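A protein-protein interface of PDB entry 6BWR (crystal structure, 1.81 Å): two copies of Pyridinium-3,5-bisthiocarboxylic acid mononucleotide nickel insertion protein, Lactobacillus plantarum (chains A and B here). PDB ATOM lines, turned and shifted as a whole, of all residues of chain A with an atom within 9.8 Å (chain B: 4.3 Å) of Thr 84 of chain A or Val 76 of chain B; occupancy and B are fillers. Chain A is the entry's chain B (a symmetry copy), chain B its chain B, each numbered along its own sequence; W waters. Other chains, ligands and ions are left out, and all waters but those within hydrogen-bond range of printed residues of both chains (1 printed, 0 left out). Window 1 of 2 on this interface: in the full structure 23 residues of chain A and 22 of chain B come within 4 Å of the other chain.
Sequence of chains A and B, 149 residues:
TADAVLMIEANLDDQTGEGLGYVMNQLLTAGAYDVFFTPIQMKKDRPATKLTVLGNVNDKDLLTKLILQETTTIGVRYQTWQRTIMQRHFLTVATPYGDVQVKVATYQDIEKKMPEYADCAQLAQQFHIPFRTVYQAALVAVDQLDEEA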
ATOM      1  N   THR A   1     -19.443  13.216  14.044  1.00  0.00           N
ATOM      2  CA  THR A   1     -20.855  13.563  14.011  1.00  0.00           C
ATOM      3  C   THR A   1     -21.246  14.158  12.639  1.00  0.00           C
ATOM      4  O   THR A   1     -20.389  14.420  11.783  1.00  0.00           O
ATOM      5  CB  THR A   1     -21.206  14.537  15.157  1.00  0.00           C
ATOM      6  OG1 THR A   1     -22.494  15.114  14.926  1.00  0.00           O
ATOM      7  CG2 THR A   1     -20.168  15.640  15.278  1.00  0.00           C
ATOM      8  N   ALA A   2     -22.551  14.323  12.426  1.00  0.00           N
ATOM      9  CA  ALA A   2     -23.112  14.865  11.197  1.00  0.00           C
ATOM     10  C   ALA A   2     -23.613  16.287  11.410  1.00  0.00           C
ATOM     11  O   ALA A   2     -24.006  16.672  12.515  1.00  0.00           O
ATOM     12  CB  ALA A   2     -24.255  13.988  10.675  1.00  0.00           C
ATOM     13  N   ASP A   3     -23.597  17.064  10.338  1.00  0.00           N
ATOM     14  CA  ASP A   3     -23.884  18.486  10.411  1.00  0.00           C
ATOM     15  C   ASP A   3     -24.301  18.964   9.027  1.00  0.00           C
ATOM     16  O   ASP A   3     -24.298  18.207   8.055  1.00  0.00           O
ATOM     17  CB  ASP A   3     -22.670  19.265  10.929  1.00  0.00           C
ATOM     18  CG  ASP A   3     -23.028  20.661  11.421  1.00  0.00           C
ATOM     19  OD1 ASP A   3     -23.947  20.787  12.261  1.00  0.00           O
ATOM     20  OD2 ASP A   3     -22.394  21.636  10.951  1.00  0.00           O
ATOM     21  N   ALA A   4     -24.693  20.225   8.956  1.00  0.00           N
ATOM     22  CA  ALA A   4     -24.869  20.906   7.688  1.00  0.00           C
ATOM     23  C   ALA A   4     -24.237  22.273   7.845  1.00  0.00           C
ATOM     24  O   ALA A   4     -24.230  22.856   8.935  1.00  0.00           O
ATOM     25  CB  ALA A   4     -26.338  21.027   7.268  1.00  0.00           C
ATOM     26  N   VAL A   5     -23.688  22.777   6.750  1.00  0.00           N
ATOM     27  CA  VAL A   5     -22.925  24.009   6.788  1.00  0.00           C
ATOM     28  C   VAL A   5     -23.357  24.879   5.623  1.00  0.00           C
ATOM     29  O   VAL A   5     -23.639  24.392   4.524  1.00  0.00           O
ATOM     30  CB  VAL A   5     -21.413  23.709   6.769  1.00  0.00           C
ATOM     31  CG1 VAL A   5     -20.995  23.103   5.449  1.00  0.00           C
ATOM     32  CG2 VAL A   5     -20.609  24.932   7.110  1.00  0.00           C
ATOM     33  N   MET A   7     -22.546  27.667   2.845  1.00  0.00           N
ATOM     34  CA  MET A   7     -21.450  28.261   2.102  1.00  0.00           C
ATOM     35  C   MET A   7     -21.962  29.514   1.423  1.00  0.00           C
ATOM     36  O   MET A   7     -22.947  29.453   0.690  1.00  0.00           O
ATOM     37  CB  MET A   7     -20.887  27.297   1.058  1.00  0.00           C
ATOM     38  CG  MET A   7     -19.720  27.888   0.257  1.00  0.00           C
ATOM     39  SD  MET A   7     -19.019  26.781  -0.985  1.00  0.00           S
ATOM     40  CE  MET A   7     -18.353  25.502   0.051  1.00  0.00           C
ATOM     41  N   LEU A  54     -17.828  29.979   5.355  1.00  0.00           N
ATOM     42  CA  LEU A  54     -18.580  28.830   5.835  1.00  0.00           C
ATOM     43  C   LEU A  54     -19.171  29.163   7.196  1.00  0.00           C
ATOM     44  O   LEU A  54     -18.536  29.829   8.013  1.00  0.00           O
ATOM     45  CB  LEU A  54     -17.693  27.594   5.904  1.00  0.00           C
ATOM     46  CG  LEU A  54     -17.234  27.159   4.508  1.00  0.00           C
ATOM     47  CD1 LEU A  54     -15.892  26.489   4.602  1.00  0.00           C
ATOM     48  CD2 LEU A  54     -18.250  26.238   3.853  1.00  0.00           C
ATOM     49  N   TRP A  81     -24.062  22.623   2.460  1.00  0.00           N
ATOM     50  CA  TRP A  81     -23.310  21.391   2.285  1.00  0.00           C
ATOM     51  C   TRP A  81     -23.556  20.479   3.475  1.00  0.00           C
ATOM     52  O   TRP A  81     -23.881  20.935   4.567  1.00  0.00           O
ATOM     53  CB  TRP A  81     -21.808  21.679   2.168  1.00  0.00           C
ATOM     54  CG  TRP A  81     -21.378  22.408   0.922  1.00  0.00           C
ATOM     55  CD1 TRP A  81     -21.810  23.632   0.488  1.00  0.00           C
ATOM     56  CD2 TRP A  81     -20.424  21.958  -0.045  1.00  0.00           C
ATOM     57  NE1 TRP A  81     -21.190  23.960  -0.691  1.00  0.00           N
ATOM     58  CE2 TRP A  81     -20.335  22.945  -1.038  1.00  0.00           C
ATOM     59  CE3 TRP A  81     -19.628  20.817  -0.163  1.00  0.00           C
ATOM     60  CZ2 TRP A  81     -19.483  22.818  -2.135  1.00  0.00           C
ATOM     61  CZ3 TRP A  81     -18.794  20.698  -1.255  1.00  0.00           C
ATOM     62  CH2 TRP A  81     -18.724  21.686  -2.216  1.00  0.00           C
ATOM     63  N   GLN A  82     -23.394  19.183   3.255  1.00  0.00           N
ATOM     64  CA  GLN A  82     -23.381  18.242   4.353  1.00  0.00           C
ATOM     65  C   GLN A  82     -21.952  18.146   4.858  1.00  0.00           C
ATOM     66  O   GLN A  82     -21.012  18.459   4.141  1.00  0.00           O
ATOM     67  CB  GLN A  82     -23.864  16.862   3.910  1.00  0.00           C
ATOM     68  CG  GLN A  82     -25.145  16.817   3.097  1.00  0.00           C
ATOM     69  CD  GLN A  82     -26.341  17.262   3.886  1.00  0.00           C
ATOM     70  OE1 GLN A  82     -26.468  16.932   5.058  1.00  0.00           O
ATOM     71  NE2 GLN A  82     -27.246  18.006   3.243  1.00  0.00           N
ATOM     72  N   ARG A  83     -21.793  17.710   6.106  1.00  0.00           N
ATOM     73  CA  ARG A  83     -20.471  17.601   6.715  1.00  0.00           C
ATOM     74  C   ARG A  83     -20.334  16.285   7.458  1.00  0.00           C
ATOM     75  O   ARG A  83     -21.261  15.848   8.142  1.00  0.00           O
ATOM     76  CB  ARG A  83     -20.194  18.741   7.716  1.00  0.00           C
ATOM     77  CG  ARG A  83     -19.777  20.053   7.111  1.00  0.00           C
ATOM     78  CD  ARG A  83     -19.092  20.938   8.132  1.00  0.00           C
ATOM     79  NE  ARG A  83     -19.896  21.103   9.333  1.00  0.00           N
ATOM     80  CZ  ARG A  83     -19.445  21.678  10.436  1.00  0.00           C
ATOM     81  NH1 ARG A  83     -18.206  22.130  10.471  1.00  0.00           N
ATOM     82  NH2 ARG A  83     -20.212  21.788  11.506  1.00  0.00           N
ATOM     83  N   THR A  84     -19.152  15.695   7.367  1.00  0.00           N
ATOM     84  CA  THR A  84     -18.756  14.571   8.198  1.00  0.00           C
ATOM     85  C   THR A  84     -17.612  15.055   9.074  1.00  0.00           C
ATOM     86  O   THR A  84     -16.617  15.563   8.557  1.00  0.00           O
ATOM     87  CB  THR A  84     -18.322  13.390   7.341  1.00  0.00           C
ATOM     88  OG1 THR A  84     -19.440  12.930   6.588  1.00  0.00           O
ATOM     89  CG2 THR A  84     -17.826  12.257   8.220  1.00  0.00           C
ATOM     90  N   ILE A  85     -17.762  14.915  10.390  1.00  0.00           N
ATOM     91  CA  ILE A  85     -16.847  15.486  11.371  1.00  0.00           C
ATOM     92  C   ILE A  85     -16.244  14.351  12.189  1.00  0.00           C
ATOM     93  O   ILE A  85     -16.947  13.407  12.568  1.00  0.00           O
ATOM     94  CB  ILE A  85     -17.575  16.483  12.295  1.00  0.00           C
ATOM     95  CG1 ILE A  85     -18.178  17.633  11.505  1.00  0.00           C
ATOM     96  CG2 ILE A  85     -16.624  17.052  13.334  1.00  0.00           C
ATOM     97  CD1 ILE A  85     -17.299  18.835  11.447  1.00  0.00           C
ATOM     98  N   MET A  86     -14.936  14.421  12.432  1.00  0.00           N
ATOM     99  CA  MET A  86     -14.321  13.488  13.364  1.00  0.00           C
ATOM    100  C   MET A  86     -14.657  13.848  14.811  1.00  0.00           C
ATOM    101  O   MET A  86     -15.020  14.978  15.141  1.00  0.00           O
ATOM    102  CB  MET A  86     -12.804  13.444  13.186  1.00  0.00           C
ATOM    103  CG  MET A  86     -12.375  13.274  11.773  1.00  0.00           C
ATOM    104  SD  MET A  86     -10.608  13.239  11.647  1.00  0.00           S
ATOM    105  CE  MET A  86     -10.294  11.573  12.184  1.00  0.00           C
ATOM    106  N   GLN A  87     -14.548  12.845  15.674  1.00  0.00           N
ATOM    107  CA  GLN A  87     -14.695  13.060  17.107  1.00  0.00           C
ATOM    108  C   GLN A  87     -13.386  13.583  17.690  1.00  0.00           C
ATOM    109  O   GLN A  87     -12.304  13.114  17.334  1.00  0.00           O
ATOM    110  CB  GLN A  87     -15.120  11.758  17.784  1.00  0.00           C
ATOM    111  CG  GLN A  87     -16.611  11.454  17.606  1.00  0.00           C
ATOM    112  CD  GLN A  87     -17.494  12.187  18.604  1.00  0.00           C
ATOM    113  OE1 GLN A  87     -17.215  12.200  19.806  1.00  0.00           O
ATOM    114  NE2 GLN A  87     -18.572  12.795  18.112  1.00  0.00           N
ATOM    115  N   ARG A  88     -13.476  14.545  18.600  1.00  0.00           N
ATOM    116  CA  ARG A  88     -12.288  15.187  19.148  1.00  0.00           C
ATOM    117  C   ARG A  88     -12.143  14.853  20.615  1.00  0.00           C
ATOM    118  O   ARG A  88     -13.136  14.727  21.335  1.00  0.00           O
ATOM    119  CB  ARG A  88     -12.297  16.722  19.063  1.00  0.00           C
ATOM    120  CG  ARG A  88     -12.564  17.386  17.761  1.00  0.00           C
ATOM    121  CD  ARG A  88     -12.790  18.885  18.017  1.00  0.00           C
ATOM    122  NE  ARG A  88     -11.968  19.695  17.114  1.00  0.00           N
ATOM    123  CZ  ARG A  88     -12.446  20.559  16.215  1.00  0.00           C
ATOM    124  NH1 ARG A  88     -13.765  20.743  16.090  1.00  0.00           N
ATOM    125  NH2 ARG A  88     -11.605  21.227  15.432  1.00  0.00           N
ATOM    126  N   THR A 106     -10.495  11.150  15.979  1.00  0.00           N
ATOM    127  CA  THR A 106     -10.795   9.753  15.712  1.00  0.00           C
ATOM    128  C   THR A 106     -12.004   9.627  14.790  1.00  0.00           C
ATOM    129  O   THR A 106     -12.927  10.445  14.821  1.00  0.00           O
ATOM    130  CB  THR A 106     -11.028   8.956  17.009  1.00  0.00           C
ATOM    131  OG1 THR A 106     -12.071   9.563  17.773  1.00  0.00           O
ATOM    132  CG2 THR A 106      -9.754   8.887  17.842  1.00  0.00           C
ATOM    133  N   TYR A 107     -11.965   8.627  13.924  1.00  0.00           N
ATOM    134  CA  TYR A 107     -13.089   8.352  13.034  1.00  0.00           C
ATOM    135  C   TYR A 107     -13.043   6.878  12.656  1.00  0.00           C
ATOM    136  O   TYR A 107     -12.142   6.451  11.933  1.00  0.00           O
ATOM    137  CB  TYR A 107     -13.036   9.247  11.803  1.00  0.00           C
ATOM    138  CG  TYR A 107     -14.250   9.097  10.934  1.00  0.00           C
ATOM    139  CD1 TYR A 107     -15.448   9.718  11.269  1.00  0.00           C
ATOM    140  CD2 TYR A 107     -14.207   8.312   9.791  1.00  0.00           C
ATOM    141  CE1 TYR A 107     -16.559   9.575  10.481  1.00  0.00           C
ATOM    142  CE2 TYR A 107     -15.314   8.156   8.997  1.00  0.00           C
ATOM    143  CZ  TYR A 107     -16.490   8.792   9.344  1.00  0.00           C
ATOM    144  OH  TYR A 107     -17.600   8.644   8.544  1.00  0.00           O
ATOM    145  N   GLN A 108     -13.999   6.102  13.151  1.00  0.00           N
ATOM    146  CA  GLN A 108     -13.964   4.668  12.923  1.00  0.00           C
ATOM    147  C   GLN A 108     -12.615   4.128  13.376  1.00  0.00           C
ATOM    148  O   GLN A 108     -12.289   4.164  14.566  1.00  0.00           O
ATOM    149  CB  GLN A 108     -14.228   4.341  11.456  1.00  0.00           C
ATOM    150  CG  GLN A 108     -15.572   4.844  10.976  1.00  0.00           C
ATOM    151  CD  GLN A 108     -15.897   4.403   9.575  1.00  0.00           C
ATOM    152  OE1 GLN A 108     -15.181   3.599   8.978  1.00  0.00           O
ATOM    153  NE2 GLN A 108     -16.974   4.939   9.032  1.00  0.00           N
ATOM    154  N   ILE A 110      -9.756   5.430  12.510  1.00  0.00           N
ATOM    155  CA  ILE A 110      -8.772   6.496  12.339  1.00  0.00           C
ATOM    156  C   ILE A 110      -8.438   7.111  13.682  1.00  0.00           C
ATOM    157  O   ILE A 110      -9.337   7.485  14.434  1.00  0.00           O
ATOM    158  CB  ILE A 110      -9.300   7.587  11.390  1.00  0.00           C
ATOM    159  CG1 ILE A 110      -9.692   6.991  10.028  1.00  0.00           C
ATOM    160  CG2 ILE A 110      -8.306   8.740  11.316  1.00  0.00           C
ATOM    161  CD1 ILE A 110     -10.595   7.883   9.190  1.00  0.00           C
ATOM    162  N   LYS A 112      -5.594  10.151  14.899  1.00  0.00           N
ATOM    163  CA  LYS A 112      -4.488  11.024  14.548  1.00  0.00           C
ATOM    164  C   LYS A 112      -4.347  12.092  15.609  1.00  0.00           C
ATOM    165  O   LYS A 112      -5.299  12.425  16.311  1.00  0.00           O
ATOM    166  CB  LYS A 112      -4.674  11.682  13.178  1.00  0.00           C
ATOM    167  CG  LYS A 112      -5.879  12.574  13.022  1.00  0.00           C
ATOM    168  CD  LYS A 112      -6.061  12.918  11.555  1.00  0.00           C
ATOM    169  CE  LYS A 112      -7.226  13.871  11.336  1.00  0.00           C
ATOM    170  NZ  LYS A 112      -7.632  13.944   9.910  1.00  0.00           N
ATOM    171  N   ILE B   8     -16.475  16.358  -2.688  1.00  0.00           N
ATOM    172  CA  ILE B   8     -15.993  16.467  -1.316  1.00  0.00           C
ATOM    173  C   ILE B   8     -14.864  17.485  -1.298  1.00  0.00           C
ATOM    174  O   ILE B   8     -13.992  17.464  -2.174  1.00  0.00           O
ATOM    175  CB  ILE B   8     -15.510  15.120  -0.752  1.00  0.00           C
ATOM    176  CG1 ILE B   8     -16.561  14.033  -0.904  1.00  0.00           C
ATOM    177  CG2 ILE B   8     -15.101  15.251   0.712  1.00  0.00           C
ATOM    178  CD1 ILE B   8     -16.020  12.722  -0.521  1.00  0.00           C
ATOM    179  N   GLU B   9     -14.904  18.393  -0.324  1.00  0.00           N
ATOM    180  CA  GLU B   9     -13.922  19.458  -0.173  1.00  0.00           C
ATOM    181  C   GLU B   9     -13.373  19.482   1.247  1.00  0.00           C
ATOM    182  O   GLU B   9     -14.049  19.097   2.202  1.00  0.00           O
ATOM    183  CB  GLU B   9     -14.501  20.851  -0.476  1.00  0.00           C
ATOM    184  CG  GLU B   9     -14.799  21.167  -1.926  1.00  0.00           C
ATOM    185  CD  GLU B   9     -15.035  22.668  -2.166  1.00  0.00           C
ATOM    186  OE1 GLU B   9     -15.209  23.436  -1.192  1.00  0.00           O
ATOM    187  OE2 GLU B   9     -15.059  23.089  -3.334  1.00  0.00           O
ATOM    188  N   THR B  64     -14.304   9.905   1.932  1.00  0.00           N
ATOM    189  CA  THR B  64     -14.296  10.661   3.180  1.00  0.00           C
ATOM    190  C   THR B  64     -13.284  10.084   4.157  1.00  0.00           C
ATOM    191  O   THR B  64     -12.455  10.808   4.717  1.00  0.00           O
ATOM    192  CB  THR B  64     -15.691  10.648   3.798  1.00  0.00           C
ATOM    193  OG1 THR B  64     -16.595  11.373   2.954  1.00  0.00           O
ATOM    194  CG2 THR B  64     -15.667  11.291   5.181  1.00  0.00           C
ATOM    195  N   ILE B  67      -9.778  10.838   3.177  1.00  0.00           N
ATOM    196  CA  ILE B  67      -9.351  12.209   3.459  1.00  0.00           C
ATOM    197  C   ILE B  67      -9.103  12.408   4.950  1.00  0.00           C
ATOM    198  O   ILE B  67      -8.115  13.034   5.350  1.00  0.00           O
ATOM    199  CB  ILE B  67     -10.388  13.211   2.934  1.00  0.00           C
ATOM    200  CG1 ILE B  67     -10.430  13.196   1.406  1.00  0.00           C
ATOM    201  CG2 ILE B  67     -10.053  14.609   3.406  1.00  0.00           C
ATOM    202  CD1 ILE B  67     -11.626  13.897   0.858  1.00  0.00           C
ATOM    203  N   LEU B  68      -9.997  11.884   5.797  1.00  0.00           N
ATOM    204  CA  LEU B  68      -9.853  12.046   7.244  1.00  0.00           C
ATOM    205  C   LEU B  68      -8.670  11.265   7.786  1.00  0.00           C
ATOM    206  O   LEU B  68      -8.064  11.658   8.790  1.00  0.00           O
ATOM    207  CB  LEU B  68     -11.128  11.606   7.950  1.00  0.00           C
ATOM    208  CG  LEU B  68     -12.354  12.410   7.560  1.00  0.00           C
ATOM    209  CD1 LEU B  68     -13.559  11.832   8.283  1.00  0.00           C
ATOM    210  CD2 LEU B  68     -12.120  13.847   7.916  1.00  0.00           C
ATOM    211  N   ILE B  74     -10.302  17.961  10.374  1.00  0.00           N
ATOM    212  CA  ILE B  74     -11.257  17.360  11.303  1.00  0.00           C
ATOM    213  C   ILE B  74     -12.587  17.035  10.625  1.00  0.00           C
ATOM    214  O   ILE B  74     -13.370  16.228  11.139  1.00  0.00           O
ATOM    215  CB  ILE B  74     -11.459  18.288  12.512  1.00  0.00           C
ATOM    216  CG1 ILE B  74     -10.113  18.564  13.154  1.00  0.00           C
ATOM    217  CG2 ILE B  74     -12.332  17.653  13.565  1.00  0.00           C
ATOM    218  CD1 ILE B  74      -9.458  17.302  13.665  1.00  0.00           C
ATOM    219  N   GLY B  75     -12.875  17.647   9.488  1.00  0.00           N
ATOM    220  CA  GLY B  75     -14.133  17.405   8.811  1.00  0.00           C
ATOM    221  C   GLY B  75     -13.998  17.625   7.322  1.00  0.00           C
ATOM    222  O   GLY B  75     -13.033  18.216   6.834  1.00  0.00           O
ATOM    223  N   VAL B  76     -14.978  17.110   6.606  1.00  0.00           N
ATOM    224  CA  VAL B  76     -15.114  17.310   5.177  1.00  0.00           C
ATOM    225  C   VAL B  76     -16.521  17.832   4.936  1.00  0.00           C
ATOM    226  O   VAL B  76     -17.435  17.583   5.724  1.00  0.00           O
ATOM    227  CB  VAL B  76     -14.870  16.012   4.378  1.00  0.00           C
ATOM    228  CG1 VAL B  76     -13.431  15.591   4.482  1.00  0.00           C
ATOM    229  CG2 VAL B  76     -15.763  14.915   4.872  1.00  0.00           C
ATOM    230  N   ARG B  77     -16.697  18.562   3.848  1.00  0.00           N
ATOM    231  CA  ARG B  77     -18.020  18.953   3.403  1.00  0.00           C
ATOM    232  C   ARG B  77     -18.285  18.321   2.043  1.00  0.00           C
ATOM    233  O   ARG B  77     -17.357  18.092   1.271  1.00  0.00           O
ATOM    234  CB  ARG B  77     -18.171  20.475   3.330  1.00  0.00           C
ATOM    235  CG  ARG B  77     -17.150  21.184   2.444  1.00  0.00           C
ATOM    236  CD  ARG B  77     -17.338  22.696   2.453  1.00  0.00           C
ATOM    237  NE  ARG B  77     -16.317  23.362   1.656  1.00  0.00           N
ATOM    238  CZ  ARG B  77     -15.111  23.668   2.121  1.00  0.00           C
ATOM    239  NH1 ARG B  77     -14.795  23.382   3.375  1.00  0.00           N
ATOM    240  NH2 ARG B  77     -14.222  24.266   1.345  1.00  0.00           N
ATOM    241  N   TYR B  78     -19.548  18.001   1.758  1.00  0.00           N
ATOM    242  CA  TYR B  78     -19.838  17.345   0.491  1.00  0.00           C
ATOM    243  C   TYR B  78     -21.213  17.751  -0.014  1.00  0.00           C
ATOM    244  O   TYR B  78     -22.097  18.119   0.764  1.00  0.00           O
ATOM    245  CB  TYR B  78     -19.720  15.813   0.588  1.00  0.00           C
ATOM    246  CG  TYR B  78     -20.622  15.166   1.583  1.00  0.00           C
ATOM    247  CD1 TYR B  78     -21.912  14.825   1.242  1.00  0.00           C
ATOM    248  CD2 TYR B  78     -20.185  14.876   2.860  1.00  0.00           C
ATOM    249  CE1 TYR B  78     -22.753  14.224   2.146  1.00  0.00           C
ATOM    250  CE2 TYR B  78     -21.018  14.278   3.772  1.00  0.00           C
ATOM    251  CZ  TYR B  78     -22.306  13.958   3.410  1.00  0.00           C
ATOM    252  OH  TYR B  78     -23.158  13.356   4.305  1.00  0.00           O
HETATM  253  O   HOH W   1     -18.959  11.155   4.804  1.00  0.00           O
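Val 5 of chain A touches none of the printed residues of chain B.
Printed residues of chain B within 4 Å of Met 7 of chain A: Glu 9 (3.96 Å) and Arg 77 (3.4 Å).
Ile 8 of chain B touches none of the printed residues of chain A.
Of the printed residues of chain A, Ile 74 of chain B touches Ile 85 (3.6 Å), Met 86 (2.7 Å) and Arg 88 (3.8 Å).
The nearest residue of chain B that does not touch Thr 84 of chain A is Ile 74 of chain B (4.2 Å).
The nearest printed residue of chain A that does not touch Val 76 of chain B is Gln 82 of chain A (4.01 Å).
No position is printed for both chains.
Met 7 of chain A touches Arg 77 of chain B (CE to NE, 3.4 Å).
Leu 54 of chain A touches Arg 77 of chain B.
C of Arg 77 of chain B touches CE3 of Trp 81 of chain A, at 3.6 Å.
N of Tyr 78 of chain B touches CE3 of Trp 81 of chain A, 3.4 Å away.
Gln 82 of chain A touches Arg 77 of chain B.
Gly 75 of chain B touches Thr 84 of chain A.
Ile 85 of chain A touches Ile 74 of chain B (CA to O, 3.6 Å).
NH2 of Arg 88 of chain A touches CG1 of Ile 74 of chain B, 3.8 Å away.
Tyr 107 of chain A touches Leu 68 of chain B (CG to CD1, 3.9 Å).
O of Leu 68 of chain B touches CG2 of Ile 110 of chain A, at 3.9 Å.
The guanidinium group of Arg 83 of chain A lies within salt-bridge range of the side-chain carboxylate of Asp 3 of chain A.
The side-chain sulfur (SD) of Met 7 of chain A lies close to the indole nitrogen (NE1) of Trp 81 of chain A.
O of Ile 85 of chain A lies within hydrogen-bond range of N of Thr 1 of chain A (2.9 Å).
The backbone carbonyl oxygen (O) of Val 5 of chain A is in hydrogen-bond range of the backbone NH (N) of Trp 81 of chain A (2.8 Å).
The side-chain sulfur (SD) of Met 86 of chain A lies close to the side-chain amino group (NZ) of Lys 112 of chain A.
NH2 of Arg 77 of chain B is in salt-bridge range of OE1 of Glu 9 of chain B (2.8 Å).
Water W1 bridges OG1 of Thr 84 of chain A (2.6 Å) and OG1 of Thr 64 of chain B (3.0 Å).
Printed residues of chain B that touch a printed residue of chain A: Glu 9, Thr 64, Leu 68, Ile 74, Gly 75, Val 76, Arg 77 and Tyr 78.
Hydrophobic or aromatic side chains of chain B that line the printed part of chain A: Leu 68, Ile 74, Val 76 and Tyr 78.
Among the printed residues, no Asp or Glu carboxylate lies within 4 Å of a Lys or Arg side-chain nitrogen of the other chain.
O of Ile 74 of chain B lies within hydrogen-bond range of N of Met 86 of chain A (2.7 Å).
The backbone carbonyl oxygen of Thr 84 of chain A sits at hydrogen-bond distance from the backbone NH of Val 76 of chain B, at 3.0 Å.
The backbone NH of Tyr 78 of chain B lies within hydrogen-bond range of the backbone carbonyl oxygen of Gln 82 of chain A (2.8 Å).
The side-chain amino group of Lys 112 of chain A sits at hydrogen-bond distance from the backbone carbonyl oxygen of Leu 68 of chain B (2.6 Å).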
